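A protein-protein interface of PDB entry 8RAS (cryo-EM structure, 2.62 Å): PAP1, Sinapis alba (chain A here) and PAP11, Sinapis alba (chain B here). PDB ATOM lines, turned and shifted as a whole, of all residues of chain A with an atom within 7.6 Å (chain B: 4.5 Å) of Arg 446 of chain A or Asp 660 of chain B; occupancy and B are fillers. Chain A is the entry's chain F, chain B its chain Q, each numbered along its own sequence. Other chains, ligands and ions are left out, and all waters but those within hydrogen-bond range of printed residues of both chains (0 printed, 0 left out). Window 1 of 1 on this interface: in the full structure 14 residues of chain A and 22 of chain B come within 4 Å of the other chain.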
ATOM      1  N   ARG A 407      13.156 -23.611  16.069  1.00  0.00           N
ATOM      2  CA  ARG A 407      12.113 -23.058  16.925  1.00  0.00           C
ATOM      3  C   ARG A 407      11.743 -24.017  18.049  1.00  0.00           C
ATOM      4  O   ARG A 407      11.573 -23.600  19.201  1.00  0.00           O
ATOM      5  CB  ARG A 407      10.881 -22.712  16.089  1.00  0.00           C
ATOM      6  CG  ARG A 407       9.597 -22.646  16.891  1.00  0.00           C
ATOM      7  CD  ARG A 407       9.451 -21.322  17.609  1.00  0.00           C
ATOM      8  NE  ARG A 407       8.053 -21.004  17.871  1.00  0.00           N
ATOM      9  CZ  ARG A 407       7.612 -20.448  18.990  1.00  0.00           C
ATOM     10  NH1 ARG A 407       8.436 -20.140  19.978  1.00  0.00           N
ATOM     11  NH2 ARG A 407       6.313 -20.199  19.123  1.00  0.00           N
ATOM     12  N   ARG A 435      13.178 -23.003  29.817  1.00  0.00           N
ATOM     13  CA  ARG A 435      13.456 -22.457  28.492  1.00  0.00           C
ATOM     14  C   ARG A 435      13.428 -20.934  28.508  1.00  0.00           C
ATOM     15  O   ARG A 435      14.295 -20.283  27.914  1.00  0.00           O
ATOM     16  CB  ARG A 435      12.448 -22.998  27.477  1.00  0.00           C
ATOM     17  CG  ARG A 435      12.778 -24.384  26.945  1.00  0.00           C
ATOM     18  CD  ARG A 435      11.751 -24.837  25.917  1.00  0.00           C
ATOM     19  NE  ARG A 435      12.007 -26.193  25.445  1.00  0.00           N
ATOM     20  CZ  ARG A 435      11.260 -26.830  24.552  1.00  0.00           C
ATOM     21  NH1 ARG A 435      10.198 -26.260  24.008  1.00  0.00           N
ATOM     22  NH2 ARG A 435      11.585 -28.069  24.200  1.00  0.00           N
ATOM     23  N   TYR A 436      12.440 -20.348  29.187  1.00  0.00           N
ATOM     24  CA  TYR A 436      12.359 -18.893  29.269  1.00  0.00           C
ATOM     25  C   TYR A 436      13.546 -18.316  30.034  1.00  0.00           C
ATOM     26  O   TYR A 436      14.086 -17.270  29.656  1.00  0.00           O
ATOM     27  CB  TYR A 436      11.035 -18.485  29.917  1.00  0.00           C
ATOM     28  CG  TYR A 436      10.715 -17.006  29.836  1.00  0.00           C
ATOM     29  CD1 TYR A 436       9.727 -16.540  28.980  1.00  0.00           C
ATOM     30  CD2 TYR A 436      11.373 -16.082  30.639  1.00  0.00           C
ATOM     31  CE1 TYR A 436       9.423 -15.194  28.906  1.00  0.00           C
ATOM     32  CE2 TYR A 436      11.075 -14.736  30.571  1.00  0.00           C
ATOM     33  CZ  TYR A 436      10.098 -14.299  29.705  1.00  0.00           C
ATOM     34  OH  TYR A 436       9.799 -12.958  29.638  1.00  0.00           O
ATOM     35  N   VAL A 437      13.964 -18.982  31.112  1.00  0.00           N
ATOM     36  CA  VAL A 437      15.059 -18.457  31.923  1.00  0.00           C
ATOM     37  C   VAL A 437      16.384 -18.549  31.172  1.00  0.00           C
ATOM     38  O   VAL A 437      17.187 -17.608  31.187  1.00  0.00           O
ATOM     39  CB  VAL A 437      15.117 -19.192  33.275  1.00  0.00           C
ATOM     40  CG1 VAL A 437      16.447 -18.940  33.969  1.00  0.00           C
ATOM     41  CG2 VAL A 437      13.960 -18.758  34.161  1.00  0.00           C
ATOM     42  N   GLU A 438      16.632 -19.674  30.498  1.00  0.00           N
ATOM     43  CA  GLU A 438      17.909 -19.884  29.827  1.00  0.00           C
ATOM     44  C   GLU A 438      18.055 -19.070  28.548  1.00  0.00           C
ATOM     45  O   GLU A 438      19.176 -18.944  28.043  1.00  0.00           O
ATOM     46  CB  GLU A 438      18.096 -21.368  29.510  1.00  0.00           C
ATOM     47  CG  GLU A 438      17.227 -21.872  28.371  1.00  0.00           C
ATOM     48  CD  GLU A 438      17.446 -23.342  28.077  1.00  0.00           C
ATOM     49  OE1 GLU A 438      18.287 -23.968  28.756  1.00  0.00           O
ATOM     50  OE2 GLU A 438      16.775 -23.874  27.168  1.00  0.00           O
ATOM     51  N   GLU A 439      16.968 -18.517  28.018  1.00  0.00           N
ATOM     52  CA  GLU A 439      17.010 -17.764  26.772  1.00  0.00           C
ATOM     53  C   GLU A 439      17.290 -16.283  26.979  1.00  0.00           C
ATOM     54  O   GLU A 439      17.285 -15.525  26.004  1.00  0.00           O
ATOM     55  CB  GLU A 439      15.694 -17.936  26.007  1.00  0.00           C
ATOM     56  CG  GLU A 439      15.640 -19.192  25.156  1.00  0.00           C
ATOM     57  CD  GLU A 439      14.248 -19.483  24.633  1.00  0.00           C
ATOM     58  OE1 GLU A 439      13.365 -18.612  24.772  1.00  0.00           O
ATOM     59  OE2 GLU A 439      14.037 -20.584  24.084  1.00  0.00           O
ATOM     60  N   GLY A 440      17.532 -15.851  28.210  1.00  0.00           N
ATOM     61  CA  GLY A 440      17.813 -14.461  28.489  1.00  0.00           C
ATOM     62  C   GLY A 440      16.635 -13.634  28.949  1.00  0.00           C
ATOM     63  O   GLY A 440      16.704 -12.402  28.871  1.00  0.00           O
ATOM     64  N   GLY A 441      15.563 -14.263  29.428  1.00  0.00           N
ATOM     65  CA  GLY A 441      14.408 -13.520  29.899  1.00  0.00           C
ATOM     66  C   GLY A 441      14.627 -12.777  31.200  1.00  0.00           C
ATOM     67  O   GLY A 441      13.752 -12.003  31.602  1.00  0.00           O
ATOM     68  N   LEU A 442      15.762 -12.992  31.862  1.00  0.00           N
ATOM     69  CA  LEU A 442      16.068 -12.291  33.101  1.00  0.00           C
ATOM     70  C   LEU A 442      16.726 -10.939  32.864  1.00  0.00           C
ATOM     71  O   LEU A 442      16.469  -9.993  33.618  1.00  0.00           O
ATOM     72  CB  LEU A 442      16.981 -13.149  33.982  1.00  0.00           C
ATOM     73  CG  LEU A 442      16.639 -14.636  34.092  1.00  0.00           C
ATOM     74  CD1 LEU A 442      17.718 -15.375  34.867  1.00  0.00           C
ATOM     75  CD2 LEU A 442      15.281 -14.837  34.739  1.00  0.00           C
ATOM     76  N   THR A 443      17.566 -10.825  31.836  1.00  0.00           N
ATOM     77  CA  THR A 443      18.301  -9.598  31.557  1.00  0.00           C
ATOM     78  C   THR A 443      17.832  -8.903  30.285  1.00  0.00           C
ATOM     79  O   THR A 443      18.525  -8.009  29.789  1.00  0.00           O
ATOM     80  CB  THR A 443      19.801  -9.890  31.469  1.00  0.00           C
ATOM     81  OG1 THR A 443      20.020 -11.024  30.620  1.00  0.00           O
ATOM     82  CG2 THR A 443      20.366 -10.181  32.850  1.00  0.00           C
ATOM     83  N   GLY A 444      16.677  -9.287  29.746  1.00  0.00           N
ATOM     84  CA  GLY A 444      16.155  -8.622  28.570  1.00  0.00           C
ATOM     85  C   GLY A 444      16.870  -8.938  27.278  1.00  0.00           C
ATOM     86  O   GLY A 444      16.793  -8.151  26.332  1.00  0.00           O
ATOM     87  N   GLU A 445      17.569 -10.070  27.207  1.00  0.00           N
ATOM     88  CA  GLU A 445      18.297 -10.469  26.012  1.00  0.00           C
ATOM     89  C   GLU A 445      17.571 -11.553  25.220  1.00  0.00           C
ATOM     90  O   GLU A 445      18.180 -12.195  24.358  1.00  0.00           O
ATOM     91  CB  GLU A 445      19.703 -10.940  26.385  1.00  0.00           C
ATOM     92  CG  GLU A 445      20.498  -9.927  27.194  1.00  0.00           C
ATOM     93  CD  GLU A 445      21.873 -10.438  27.579  1.00  0.00           C
ATOM     94  OE1 GLU A 445      22.017 -11.660  27.794  1.00  0.00           O
ATOM     95  OE2 GLU A 445      22.810  -9.617  27.666  1.00  0.00           O
ATOM     96  N   ARG A 446      16.289 -11.771  25.498  1.00  0.00           N
ATOM     97  CA  ARG A 446      15.534 -12.791  24.788  1.00  0.00           C
ATOM     98  C   ARG A 446      15.246 -12.349  23.355  1.00  0.00           C
ATOM     99  O   ARG A 446      15.338 -11.170  23.006  1.00  0.00           O
ATOM    100  CB  ARG A 446      14.224 -13.097  25.517  1.00  0.00           C
ATOM    101  CG  ARG A 446      13.704 -14.508  25.290  1.00  0.00           C
ATOM    102  CD  ARG A 446      12.301 -14.690  25.841  1.00  0.00           C
ATOM    103  NE  ARG A 446      11.608 -15.800  25.199  1.00  0.00           N
ATOM    104  CZ  ARG A 446      10.502 -15.678  24.478  1.00  0.00           C
ATOM    105  NH1 ARG A 446       9.921 -14.505  24.295  1.00  0.00           N
ATOM    106  NH2 ARG A 446       9.965 -16.763  23.926  1.00  0.00           N
ATOM    107  N   LYS A 447      14.899 -13.324  22.520  1.00  0.00           N
ATOM    108  CA  LYS A 447      14.560 -13.095  21.119  1.00  0.00           C
ATOM    109  C   LYS A 447      13.058 -13.290  20.957  1.00  0.00           C
ATOM    110  O   LYS A 447      12.566 -14.423  20.984  1.00  0.00           O
ATOM    111  CB  LYS A 447      15.343 -14.039  20.209  1.00  0.00           C
ATOM    112  CG  LYS A 447      15.354 -13.624  18.750  1.00  0.00           C
ATOM    113  CD  LYS A 447      14.309 -14.383  17.951  1.00  0.00           C
ATOM    114  CE  LYS A 447      14.208 -13.844  16.536  1.00  0.00           C
ATOM    115  NZ  LYS A 447      13.058 -14.433  15.798  1.00  0.00           N
ATOM    116  N   ARG A 448      12.334 -12.187  20.785  1.00  0.00           N
ATOM    117  CA  ARG A 448      10.882 -12.234  20.697  1.00  0.00           C
ATOM    118  C   ARG A 448      10.451 -12.557  19.270  1.00  0.00           C
ATOM    119  O   ARG A 448      10.928 -11.940  18.313  1.00  0.00           O
ATOM    120  CB  ARG A 448      10.287 -10.904  21.155  1.00  0.00           C
ATOM    121  CG  ARG A 448       9.426 -11.021  22.398  1.00  0.00           C
ATOM    122  CD  ARG A 448      10.278 -11.288  23.629  1.00  0.00           C
ATOM    123  NE  ARG A 448      11.151 -10.169  23.963  1.00  0.00           N
ATOM    124  CZ  ARG A 448      10.914  -9.299  24.935  1.00  0.00           C
ATOM    125  NH1 ARG A 448       9.842  -9.398  25.704  1.00  0.00           N
ATOM    126  NH2 ARG A 448      11.775  -8.307  25.143  1.00  0.00           N
ATOM    127  N   TRP A 449       9.552 -13.528  19.132  1.00  0.00           N
ATOM    128  CA  TRP A 449       9.123 -14.019  17.821  1.00  0.00           C
ATOM    129  C   TRP A 449       7.833 -13.330  17.374  1.00  0.00           C
ATOM    130  O   TRP A 449       6.806 -13.963  17.130  1.00  0.00           O
ATOM    131  CB  TRP A 449       8.953 -15.534  17.857  1.00  0.00           C
ATOM    132  CG  TRP A 449      10.247 -16.283  17.838  1.00  0.00           C
ATOM    133  CD1 TRP A 449      11.171 -16.344  18.839  1.00  0.00           C
ATOM    134  CD2 TRP A 449      10.759 -17.081  16.767  1.00  0.00           C
ATOM    135  NE1 TRP A 449      12.231 -17.130  18.456  1.00  0.00           N
ATOM    136  CE2 TRP A 449      12.002 -17.594  17.188  1.00  0.00           C
ATOM    137  CE3 TRP A 449      10.291 -17.409  15.492  1.00  0.00           C
ATOM    138  CZ2 TRP A 449      12.781 -18.419  16.379  1.00  0.00           C
ATOM    139  CZ3 TRP A 449      11.064 -18.228  14.691  1.00  0.00           C
ATOM    140  CH2 TRP A 449      12.296 -18.724  15.137  1.00  0.00           C
ATOM    141  N   VAL A 450       7.901 -12.013  17.262  1.00  0.00           N
ATOM    142  CA  VAL A 450       6.782 -11.186  16.815  1.00  0.00           C
ATOM    143  C   VAL A 450       7.155 -10.566  15.476  1.00  0.00           C
ATOM    144  O   VAL A 450       8.266 -10.039  15.341  1.00  0.00           O
ATOM    145  CB  VAL A 450       6.430 -10.095  17.845  1.00  0.00           C
ATOM    146  CG1 VAL A 450       7.694  -9.442  18.383  1.00  0.00           C
ATOM    147  CG2 VAL A 450       5.506  -9.054  17.232  1.00  0.00           C
ATOM    148  N   PRO A 451       6.285 -10.622  14.466  1.00  0.00           N
ATOM    149  CA  PRO A 451       6.615 -10.000  13.179  1.00  0.00           C
ATOM    150  C   PRO A 451       6.761  -8.493  13.312  1.00  0.00           C
ATOM    151  O   PRO A 451       6.103  -7.851  14.132  1.00  0.00           O
ATOM    152  CB  PRO A 451       5.424 -10.371  12.286  1.00  0.00           C
ATOM    153  CG  PRO A 451       4.767 -11.528  12.968  1.00  0.00           C
ATOM    154  CD  PRO A 451       4.990 -11.317  14.431  1.00  0.00           C
ATOM    155  N   ARG A 452       7.640  -7.928  12.485  1.00  0.00           N
ATOM    156  CA  ARG A 452       7.926  -6.502  12.516  1.00  0.00           C
ATOM    157  C   ARG A 452       7.974  -5.962  11.096  1.00  0.00           C
ATOM    158  O   ARG A 452       8.281  -6.688  10.147  1.00  0.00           O
ATOM    159  CB  ARG A 452       9.249  -6.208  13.234  1.00  0.00           C
ATOM    160  CG  ARG A 452       9.147  -6.223  14.748  1.00  0.00           C
ATOM    161  CD  ARG A 452       7.943  -5.430  15.229  1.00  0.00           C
ATOM    162  NE  ARG A 452       7.460  -5.898  16.522  1.00  0.00           N
ATOM    163  CZ  ARG A 452       8.042  -5.626  17.682  1.00  0.00           C
ATOM    164  NH1 ARG A 452       9.141  -4.893  17.750  1.00  0.00           N
ATOM    165  NH2 ARG A 452       7.508  -6.103  18.803  1.00  0.00           N
ATOM    166  N   LEU B 656       3.821  -5.679  22.781  1.00  0.00           N
ATOM    167  CA  LEU B 656       3.826  -6.854  21.915  1.00  0.00           C
ATOM    168  C   LEU B 656       4.867  -7.872  22.369  1.00  0.00           C
ATOM    169  O   LEU B 656       4.611  -9.081  22.352  1.00  0.00           O
ATOM    170  CB  LEU B 656       4.072  -6.441  20.464  1.00  0.00           C
ATOM    171  CG  LEU B 656       2.859  -6.022  19.625  1.00  0.00           C
ATOM    172  CD1 LEU B 656       1.724  -7.028  19.755  1.00  0.00           C
ATOM    173  CD2 LEU B 656       2.383  -4.622  19.992  1.00  0.00           C
ATOM    174  N   ASP B 657       6.045  -7.403  22.785  1.00  0.00           N
ATOM    175  CA  ASP B 657       7.083  -8.320  23.249  1.00  0.00           C
ATOM    176  C   ASP B 657       6.673  -9.030  24.535  1.00  0.00           C
ATOM    177  O   ASP B 657       6.904 -10.236  24.690  1.00  0.00           O
ATOM    178  CB  ASP B 657       8.395  -7.561  23.446  1.00  0.00           C
ATOM    179  CG  ASP B 657       8.837  -6.826  22.198  1.00  0.00           C
ATOM    180  OD1 ASP B 657       8.459  -5.647  22.037  1.00  0.00           O
ATOM    181  OD2 ASP B 657       9.561  -7.427  21.376  1.00  0.00           O
ATOM    182  N   ILE B 658       6.059  -8.304  25.470  1.00  0.00           N
ATOM    183  CA  ILE B 658       5.593  -8.930  26.704  1.00  0.00           C
ATOM    184  C   ILE B 658       4.494  -9.943  26.403  1.00  0.00           C
ATOM    185  O   ILE B 658       4.473 -11.051  26.960  1.00  0.00           O
ATOM    186  CB  ILE B 658       5.127  -7.853  27.700  1.00  0.00           C
ATOM    187  CG1 ILE B 658       5.933  -6.569  27.504  1.00  0.00           C
ATOM    188  CG2 ILE B 658       5.289  -8.340  29.125  1.00  0.00           C
ATOM    189  CD1 ILE B 658       5.489  -5.424  28.385  1.00  0.00           C
ATOM    190  N   LEU B 659       3.572  -9.587  25.507  1.00  0.00           N
ATOM    191  CA  LEU B 659       2.513 -10.515  25.130  1.00  0.00           C
ATOM    192  C   LEU B 659       3.076 -11.749  24.436  1.00  0.00           C
ATOM    193  O   LEU B 659       2.504 -12.838  24.543  1.00  0.00           O
ATOM    194  CB  LEU B 659       1.499  -9.804  24.237  1.00  0.00           C
ATOM    195  CG  LEU B 659       0.072 -10.344  24.285  1.00  0.00           C
ATOM    196  CD1 LEU B 659      -0.346 -10.631  25.718  1.00  0.00           C
ATOM    197  CD2 LEU B 659      -0.884  -9.363  23.640  1.00  0.00           C
ATOM    198  N   ASP B 660       4.187 -11.592  23.712  1.00  0.00           N
ATOM    199  CA  ASP B 660       4.925 -12.752  23.223  1.00  0.00           C
ATOM    200  C   ASP B 660       5.456 -13.581  24.381  1.00  0.00           C
ATOM    201  O   ASP B 660       5.412 -14.817  24.346  1.00  0.00           O
ATOM    202  CB  ASP B 660       6.081 -12.302  22.331  1.00  0.00           C
ATOM    203  CG  ASP B 660       6.839 -13.465  21.735  1.00  0.00           C
ATOM    204  OD1 ASP B 660       6.349 -14.044  20.745  1.00  0.00           O
ATOM    205  OD2 ASP B 660       7.917 -13.809  22.262  1.00  0.00           O
ATOM    206  N   ASP B 661       5.980 -12.911  25.409  1.00  0.00           N
ATOM    207  CA  ASP B 661       6.480 -13.618  26.583  1.00  0.00           C
ATOM    208  C   ASP B 661       5.376 -14.403  27.280  1.00  0.00           C
ATOM    209  O   ASP B 661       5.660 -15.390  27.966  1.00  0.00           O
ATOM    210  CB  ASP B 661       7.131 -12.634  27.554  1.00  0.00           C
ATOM    211  CG  ASP B 661       8.426 -12.057  27.019  1.00  0.00           C
ATOM    212  OD1 ASP B 661       9.168 -12.795  26.337  1.00  0.00           O
ATOM    213  OD2 ASP B 661       8.702 -10.867  27.278  1.00  0.00           O
ATOM    214  N   MET B 662       4.118 -13.980  27.127  1.00  0.00           N
ATOM    215  CA  MET B 662       3.011 -14.788  27.636  1.00  0.00           C
ATOM    216  C   MET B 662       2.978 -16.164  26.982  1.00  0.00           C
ATOM    217  O   MET B 662       2.966 -17.192  27.668  1.00  0.00           O
ATOM    218  CB  MET B 662       1.674 -14.075  27.425  1.00  0.00           C
ATOM    219  CG  MET B 662       1.518 -12.741  28.126  1.00  0.00           C
ATOM    220  SD  MET B 662       2.648 -12.526  29.510  1.00  0.00           S
ATOM    221  CE  MET B 662       2.739 -10.743  29.568  1.00  0.00           C
ATOM    222  N   LEU B 663       2.981 -16.210  25.651  1.00  0.00           N
ATOM    223  CA  LEU B 663       2.820 -17.486  24.966  1.00  0.00           C
ATOM    224  C   LEU B 663       4.049 -18.379  25.074  1.00  0.00           C
ATOM    225  O   LEU B 663       3.974 -19.550  24.688  1.00  0.00           O
ATOM    226  CB  LEU B 663       2.470 -17.249  23.497  1.00  0.00           C
ATOM    227  CG  LEU B 663       1.069 -16.694  23.229  1.00  0.00           C
ATOM    228  CD1 LEU B 663       1.001 -16.033  21.864  1.00  0.00           C
ATOM    229  CD2 LEU B 663       0.030 -17.795  23.345  1.00  0.00           C
ATOM    230  N   SER B 664       5.169 -17.864  25.590  1.00  0.00           N
ATOM    231  CA  SER B 664       6.374 -18.679  25.712  1.00  0.00           C
ATOM    232  C   SER B 664       6.184 -19.832  26.689  1.00  0.00           C
ATOM    233  O   SER B 664       6.872 -20.854  26.578  1.00  0.00           O
ATOM    234  CB  SER B 664       7.553 -17.811  26.145  1.00  0.00           C
ATOM    235  OG  SER B 664       7.187 -16.951  27.209  1.00  0.00           O
ATOM    236  N   THR B 669       4.001 -18.324  20.182  1.00  0.00           N
ATOM    237  CA  THR B 669       4.539 -16.973  20.128  1.00  0.00           C
ATOM    238  C   THR B 669       3.551 -16.099  19.365  1.00  0.00           C
ATOM    239  O   THR B 669       2.510 -16.570  18.898  1.00  0.00           O
ATOM    240  CB  THR B 669       5.923 -16.941  19.473  1.00  0.00           C
ATOM    241  OG1 THR B 669       5.983 -17.916  18.425  1.00  0.00           O
ATOM    242  CG2 THR B 669       7.016 -17.218  20.497  1.00  0.00           C
ATOM    243  N   MET B 670       3.884 -14.811  19.240  1.00  0.00           N
ATOM    244  CA  MET B 670       3.035 -13.914  18.464  1.00  0.00           C
ATOM    245  C   MET B 670       2.969 -14.338  17.004  1.00  0.00           C
ATOM    246  O   MET B 670       1.930 -14.187  16.357  1.00  0.00           O
ATOM    247  CB  MET B 670       3.529 -12.472  18.574  1.00  0.00           C
ATOM    248  CG  MET B 670       3.588 -11.951  19.986  1.00  0.00           C
ATOM    249  SD  MET B 670       2.671 -10.416  20.191  1.00  0.00           S
ATOM    250  CE  MET B 670       0.992 -10.998  19.984  1.00  0.00           C
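Of the 11 printed residues of chain B, 8 touch a printed residue of chain A. Printed residues of chain A that touch a printed residue of chain B: Arg 407, Tyr 436, Arg 446, Arg 448, Trp 449, Val 450 and Arg 452. Among the printed residues, 16 pairs touch across the chains. Among the printed residues, Asp or Glu carboxylates within 4 Å of a Lys or Arg side-chain nitrogen of the other chain: Arg 446 of chain A with Asp 660 of chain B (2.9 Å), Arg 446 of chain A with Asp 661 of chain B (2.8 Å), Arg 448 of chain A with Asp 661 of chain B (2.4 Å) and Arg 452 of chain A with Asp 657 of chain B (3.4 Å).
Arg 446 of chain A touches just these residues of chain B: Asp 660, Asp 661 and Ser 664. Asp 660 of chain B touches just these residues of chain A: Arg 446, Arg 448 and Trp 449. Printed residues of chain B within 4 Å of Arg 407 of chain A: Thr 669 (2.4 Å). Printed residues of chain B within 4 Å of Val 450 of chain A: Met 670 (3.8 Å). Of the printed residues of chain B, Trp 449 of chain A touches Asp 660 (3.5 Å), Thr 669 (3.7 Å) and Met 670 (3.7 Å). Of the printed residues of chain B, Arg 452 of chain A touches Leu 656 and Asp 657. Of the printed residues of chain A, Ile 658 of chain B touches Arg 448. The nearest printed residue of chain B that does not touch Arg 446 of chain A is Thr 669 of chain B (4.5 Å). The nearest residue of chain A that does not touch Asp 660 of chain B is Val 450 of chain A (4.3 Å).
Among the printed residues, merely in contact across the chains: Tyr 436 of chain A with Ser 664 of chain B, Arg 446 of chain A with Ser 664 of chain B, Arg 448 of chain A with Ile 658 of chain B, Arg 448 of chain A with Asp 660 of chain B, Trp 449 of chain A with Asp 660 of chain B, Trp 449 of chain A with Thr 669 of chain B, Trp 449 of chain A with Met 670 of chain B, Val 450 of chain A with Met 670 of chain B and Arg 452 of chain A with Leu 656 of chain B.
OD1 of Asp 660 of chain B is in hydrogen-bond range of N of Met 670 of chain B. O of Tyr 436 of chain A sits at hydrogen-bond distance from N of Gly 441 of chain A (3.4 Å). The guanidinium group (NE) of Arg 446 of chain A is in salt-bridge range of the side-chain carboxylate (OE1) of Glu 439 of chain A, at 3.3 Å. The backbone carbonyl oxygen of Gly 440 of chain A lies within hydrogen-bond range of the backbone NH of Arg 446 of chain A (3.5 Å).
O of Asp 657 of chain B is in hydrogen-bond range of NH1 of Arg 448 of chain A, 3.2 Å away. The side-chain carboxylate (OD1) of Asp 657 of chain B lies within salt-bridge range of the guanidinium group (NH2) of Arg 452 of chain A, at 3.4 Å. The side-chain carboxylate of Asp 660 of chain B is in salt-bridge range of the guanidinium group of Arg 446 of chain A (2.9 Å). OD2 of Asp 661 of chain B sits close to OH of Tyr 436 of chain A, at 3.3 Å. The guanidinium group of Arg 446 of chain A is in salt-bridge range of the side-chain carboxylate of Asp 661 of chain B. The guanidinium group of Arg 448 of chain A is in salt-bridge range of the side-chain carboxylate of Asp 661 of chain B (2.4 Å). OG1 of Thr 669 of chain B sits at hydrogen-bond distance from NH2 of Arg 407 of chain A (2.4 Å).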
